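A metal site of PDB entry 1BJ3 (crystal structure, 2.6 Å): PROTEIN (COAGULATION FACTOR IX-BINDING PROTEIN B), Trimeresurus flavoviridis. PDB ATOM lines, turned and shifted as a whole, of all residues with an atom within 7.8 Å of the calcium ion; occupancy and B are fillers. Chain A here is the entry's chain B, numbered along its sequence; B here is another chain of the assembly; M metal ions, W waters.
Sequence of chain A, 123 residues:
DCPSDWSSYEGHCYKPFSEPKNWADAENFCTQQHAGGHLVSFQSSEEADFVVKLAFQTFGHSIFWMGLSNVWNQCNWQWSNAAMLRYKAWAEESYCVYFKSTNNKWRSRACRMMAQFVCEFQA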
ATOM      1  N   HIS A  12       7.684  15.660  -4.056  1.00  0.00           N
ATOM      2  CA  HIS A  12       6.233  15.694  -4.162  1.00  0.00           C
ATOM      3  C   HIS A  12       5.647  15.431  -2.802  1.00  0.00           C
ATOM      4  O   HIS A  12       6.308  14.803  -1.956  1.00  0.00           O
ATOM      5  CB  HIS A  12       5.716  14.662  -5.160  1.00  0.00           C
ATOM      6  CG  HIS A  12       5.916  15.063  -6.583  1.00  0.00           C
ATOM      7  ND1 HIS A  12       4.872  15.242  -7.463  1.00  0.00           N
ATOM      8  CD2 HIS A  12       7.037  15.401  -7.247  1.00  0.00           C
ATOM      9  CE1 HIS A  12       5.351  15.671  -8.621  1.00  0.00           C
ATOM     10  NE2 HIS A  12       6.659  15.774  -8.513  1.00  0.00           N
ATOM     11  N   TYR A  14       2.425  13.704  -0.740  1.00  0.00           N
ATOM     12  CA  TYR A  14       1.296  12.786  -0.748  1.00  0.00           C
ATOM     13  C   TYR A  14       0.658  12.788   0.630  1.00  0.00           C
ATOM     14  O   TYR A  14       1.337  12.787   1.648  1.00  0.00           O
ATOM     15  CB  TYR A  14       1.764  11.364  -1.058  1.00  0.00           C
ATOM     16  CG  TYR A  14       2.625  11.316  -2.275  1.00  0.00           C
ATOM     17  CD1 TYR A  14       2.065  11.181  -3.529  1.00  0.00           C
ATOM     18  CD2 TYR A  14       4.006  11.484  -2.184  1.00  0.00           C
ATOM     19  CE1 TYR A  14       2.834  11.208  -4.663  1.00  0.00           C
ATOM     20  CE2 TYR A  14       4.784  11.514  -3.318  1.00  0.00           C
ATOM     21  CZ  TYR A  14       4.193  11.375  -4.565  1.00  0.00           C
ATOM     22  OH  TYR A  14       4.931  11.371  -5.737  1.00  0.00           O
ATOM     23  N   LEU A  39      -5.644  14.394  -7.590  1.00  0.00           N
ATOM     24  CA  LEU A  39      -5.695  13.020  -7.106  1.00  0.00           C
ATOM     25  C   LEU A  39      -4.312  12.433  -7.408  1.00  0.00           C
ATOM     26  O   LEU A  39      -3.583  12.967  -8.252  1.00  0.00           O
ATOM     27  CB  LEU A  39      -6.765  12.273  -7.889  1.00  0.00           C
ATOM     28  CG  LEU A  39      -7.865  11.424  -7.226  1.00  0.00           C
ATOM     29  CD1 LEU A  39      -7.924  11.608  -5.717  1.00  0.00           C
ATOM     30  CD2 LEU A  39      -9.186  11.797  -7.874  1.00  0.00           C
ATOM     31  N   VAL A  40      -3.960  11.319  -6.769  1.00  0.00           N
ATOM     32  CA  VAL A  40      -2.651  10.693  -6.996  1.00  0.00           C
ATOM     33  C   VAL A  40      -2.381  10.047  -8.351  1.00  0.00           C
ATOM     34  O   VAL A  40      -3.118   9.170  -8.801  1.00  0.00           O
ATOM     35  CB  VAL A  40      -2.274   9.677  -5.896  1.00  0.00           C
ATOM     36  CG1 VAL A  40      -3.288   8.573  -5.796  1.00  0.00           C
ATOM     37  CG2 VAL A  40      -0.917   9.102  -6.176  1.00  0.00           C
ATOM     38  N   SER A  41      -1.323  10.505  -9.014  1.00  0.00           N
ATOM     39  CA  SER A  41      -0.886   9.982 -10.310  1.00  0.00           C
ATOM     40  C   SER A  41       0.395   9.188 -10.089  1.00  0.00           C
ATOM     41  O   SER A  41       1.389   9.787  -9.622  1.00  0.00           O
ATOM     42  CB  SER A  41      -0.582  11.134 -11.290  1.00  0.00           C
ATOM     43  OG  SER A  41       0.656  11.779 -11.010  1.00  0.00           O
ATOM     44  N   PHE A  42       0.375   7.885 -10.372  1.00  0.00           N
ATOM     45  CA  PHE A  42       1.564   7.025 -10.220  1.00  0.00           C
ATOM     46  C   PHE A  42       2.407   7.006 -11.506  1.00  0.00           C
ATOM     47  O   PHE A  42       2.057   6.339 -12.470  1.00  0.00           O
ATOM     48  CB  PHE A  42       1.154   5.604  -9.919  1.00  0.00           C
ATOM     49  CG  PHE A  42       0.528   5.424  -8.560  1.00  0.00           C
ATOM     50  CD1 PHE A  42       0.781   6.301  -7.532  1.00  0.00           C
ATOM     51  CD2 PHE A  42      -0.316   4.335  -8.323  1.00  0.00           C
ATOM     52  CE1 PHE A  42       0.209   6.095  -6.282  1.00  0.00           C
ATOM     53  CE2 PHE A  42      -0.896   4.126  -7.073  1.00  0.00           C
ATOM     54  CZ  PHE A  42      -0.629   4.994  -6.060  1.00  0.00           C
ATOM     55  N   GLN A  43       3.479   7.787 -11.536  1.00  0.00           N
ATOM     56  CA  GLN A  43       4.382   7.855 -12.688  1.00  0.00           C
ATOM     57  C   GLN A  43       5.393   6.731 -12.669  1.00  0.00           C
ATOM     58  O   GLN A  43       6.224   6.621 -13.565  1.00  0.00           O
ATOM     59  CB  GLN A  43       5.112   9.192 -12.738  1.00  0.00           C
ATOM     60  CG  GLN A  43       4.467  10.227 -13.633  1.00  0.00           C
ATOM     61  CD  GLN A  43       3.231  10.852 -13.022  1.00  0.00           C
ATOM     62  OE1 GLN A  43       2.999  10.711 -11.822  1.00  0.00           O
ATOM     63  NE2 GLN A  43       2.451  11.570 -13.820  1.00  0.00           N
ATOM     64  N   SER A  44       5.335   5.903 -11.636  1.00  0.00           N
ATOM     65  CA  SER A  44       6.253   4.790 -11.496  1.00  0.00           C
ATOM     66  C   SER A  44       5.920   3.828 -10.361  1.00  0.00           C
ATOM     67  O   SER A  44       5.026   4.064  -9.549  1.00  0.00           O
ATOM     68  CB  SER A  44       7.699   5.250 -11.383  1.00  0.00           C
ATOM     69  OG  SER A  44       7.856   6.254 -10.411  1.00  0.00           O
ATOM     70  N   GLU A  47       7.303   5.287  -6.932  1.00  0.00           N
ATOM     71  CA  GLU A  47       6.358   6.270  -6.429  1.00  0.00           C
ATOM     72  C   GLU A  47       5.117   5.564  -5.941  1.00  0.00           C
ATOM     73  O   GLU A  47       4.571   5.877  -4.880  1.00  0.00           O
ATOM     74  CB  GLU A  47       6.014   7.225  -7.547  1.00  0.00           C
ATOM     75  CG  GLU A  47       4.952   8.257  -7.254  1.00  0.00           C
ATOM     76  CD  GLU A  47       4.616   9.079  -8.489  1.00  0.00           C
ATOM     77  OE1 GLU A  47       5.270   8.878  -9.526  1.00  0.00           O
ATOM     78  OE2 GLU A  47       3.703   9.917  -8.428  1.00  0.00           O
ATOM     79  N   VAL A  51       3.546   5.346  -2.096  1.00  0.00           N
ATOM     80  CA  VAL A  51       2.177   5.682  -1.797  1.00  0.00           C
ATOM     81  C   VAL A  51       1.466   4.540  -1.102  1.00  0.00           C
ATOM     82  O   VAL A  51       0.621   4.783  -0.240  1.00  0.00           O
ATOM     83  CB  VAL A  51       1.427   6.059  -3.065  1.00  0.00           C
ATOM     84  CG1 VAL A  51      -0.041   6.226  -2.779  1.00  0.00           C
ATOM     85  CG2 VAL A  51       2.017   7.323  -3.646  1.00  0.00           C
ATOM     86  N   GLU A 120      -2.044  14.670  -4.067  1.00  0.00           N
ATOM     87  CA  GLU A 120      -0.635  15.022  -4.225  1.00  0.00           C
ATOM     88  C   GLU A 120      -0.448  16.309  -5.033  1.00  0.00           C
ATOM     89  O   GLU A 120      -1.347  16.753  -5.737  1.00  0.00           O
ATOM     90  CB  GLU A 120       0.186  13.859  -4.833  1.00  0.00           C
ATOM     91  CG  GLU A 120       0.163  13.700  -6.362  1.00  0.00           C
ATOM     92  CD  GLU A 120       1.484  13.191  -6.921  1.00  0.00           C
ATOM     93  OE1 GLU A 120       2.495  13.928  -6.841  1.00  0.00           O
ATOM     94  OE2 GLU A 120       1.527  12.061  -7.433  1.00  0.00           O
ATOM     95  N   PHE A 121       0.710  16.917  -4.841  1.00  0.00           N
ATOM     96  CA  PHE A 121       1.135  18.124  -5.547  1.00  0.00           C
ATOM     97  C   PHE A 121       2.666  18.103  -5.439  1.00  0.00           C
ATOM     98  O   PHE A 121       3.235  17.159  -4.843  1.00  0.00           O
ATOM     99  CB  PHE A 121       0.558  19.433  -4.926  1.00  0.00           C
ATOM    100  CG  PHE A 121       1.080  19.757  -3.546  1.00  0.00           C
ATOM    101  CD1 PHE A 121       2.279  20.433  -3.370  1.00  0.00           C
ATOM    102  CD2 PHE A 121       0.408  19.306  -2.420  1.00  0.00           C
ATOM    103  CE1 PHE A 121       2.827  20.630  -2.091  1.00  0.00           C
ATOM    104  CE2 PHE A 121       0.959  19.496  -1.134  1.00  0.00           C
ATOM    105  CZ  PHE A 121       2.162  20.160  -0.973  1.00  0.00           C
ATOM    106  N   TRP B  83      -3.698  11.560 -16.525  1.00  0.00           N
ATOM    107  CA  TRP B  83      -4.030  11.594 -15.115  1.00  0.00           C
ATOM    108  C   TRP B  83      -4.639  13.002 -14.905  1.00  0.00           C
ATOM    109  O   TRP B  83      -4.398  13.896 -15.734  1.00  0.00           O
ATOM    110  CB  TRP B  83      -2.755  11.455 -14.287  1.00  0.00           C
ATOM    111  CG  TRP B  83      -2.069  10.152 -14.424  1.00  0.00           C
ATOM    112  CD1 TRP B  83      -1.088   9.823 -15.306  1.00  0.00           C
ATOM    113  CD2 TRP B  83      -2.254   9.007 -13.585  1.00  0.00           C
ATOM    114  NE1 TRP B  83      -0.649   8.557 -15.074  1.00  0.00           N
ATOM    115  CE2 TRP B  83      -1.334   8.031 -14.009  1.00  0.00           C
ATOM    116  CE3 TRP B  83      -3.095   8.710 -12.505  1.00  0.00           C
ATOM    117  CZ2 TRP B  83      -1.242   6.782 -13.409  1.00  0.00           C
ATOM    118  CZ3 TRP B  83      -3.000   7.485 -11.910  1.00  0.00           C
ATOM    119  CH2 TRP B  83      -2.076   6.527 -12.348  1.00  0.00           C
ATOM    120  N   ASP B  85      -3.836  15.508 -13.185  1.00  0.00           N
ATOM    121  CA  ASP B  85      -2.864  16.605 -13.201  1.00  0.00           C
ATOM    122  C   ASP B  85      -2.386  16.968 -14.597  1.00  0.00           C
ATOM    123  O   ASP B  85      -1.577  17.875 -14.762  1.00  0.00           O
ATOM    124  CB  ASP B  85      -1.649  16.270 -12.338  1.00  0.00           C
ATOM    125  CG  ASP B  85      -0.942  15.026 -12.797  1.00  0.00           C
ATOM    126  OD1 ASP B  85      -1.362  14.443 -13.812  1.00  0.00           O
ATOM    127  OD2 ASP B  85       0.041  14.614 -12.118  1.00  0.00           O
ATOM    128  N   SER B  87      -0.846  14.656 -16.778  1.00  0.00           N
ATOM    129  CA  SER B  87       0.314  13.869 -17.188  1.00  0.00           C
ATOM    130  C   SER B  87      -0.115  12.663 -18.041  1.00  0.00           C
ATOM    131  O   SER B  87      -1.231  12.177 -17.919  1.00  0.00           O
ATOM    132  CB  SER B  87       1.074  13.319 -15.974  1.00  0.00           C
ATOM    133  OG  SER B  87       0.888  14.074 -14.788  1.00  0.00           O
HETATM  134 CA    CA M   1       2.722  11.672  -9.728  1.00  0.00          CA
HETATM  135  O   HOH W   1       2.672  13.820 -10.612  1.00  0.00           O
HETATM  136  O   HOH W   2       4.896  11.654 -10.176  1.00  0.00           O
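OE1 of Glu 120 is in hydrogen-bond range of ND1 of His 12, 2.8 Å away.
The side-chain hydroxyl of Ser 41 sits close to the side-chain carboxylate of Asp 85 of chain B (3.1 Å).
NE2 of Gln 43 lies close to OG of Ser 87 of chain B, 3.1 Å away.
OE2 of Glu 47 sits close to OH of Tyr 14, at 3.3 Å.
The nearest printed residue that does not touch the calcium ion is Phe 42 (4.5 Å).
The calcium ion is bound by water W2 (2.2 Å), the backbone carbonyl oxygen of Ser 41 (2.3 Å), the side-chain amide oxygen of Gln 43 (2.3 Å), water W1 (2.3 Å), the side-chain carboxylate of Glu 47 (2.4 Å), the side-chain hydroxyl of Ser 41 (2.4 Å) and the side-chain carboxylate of Glu 120 (2.6 Å).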
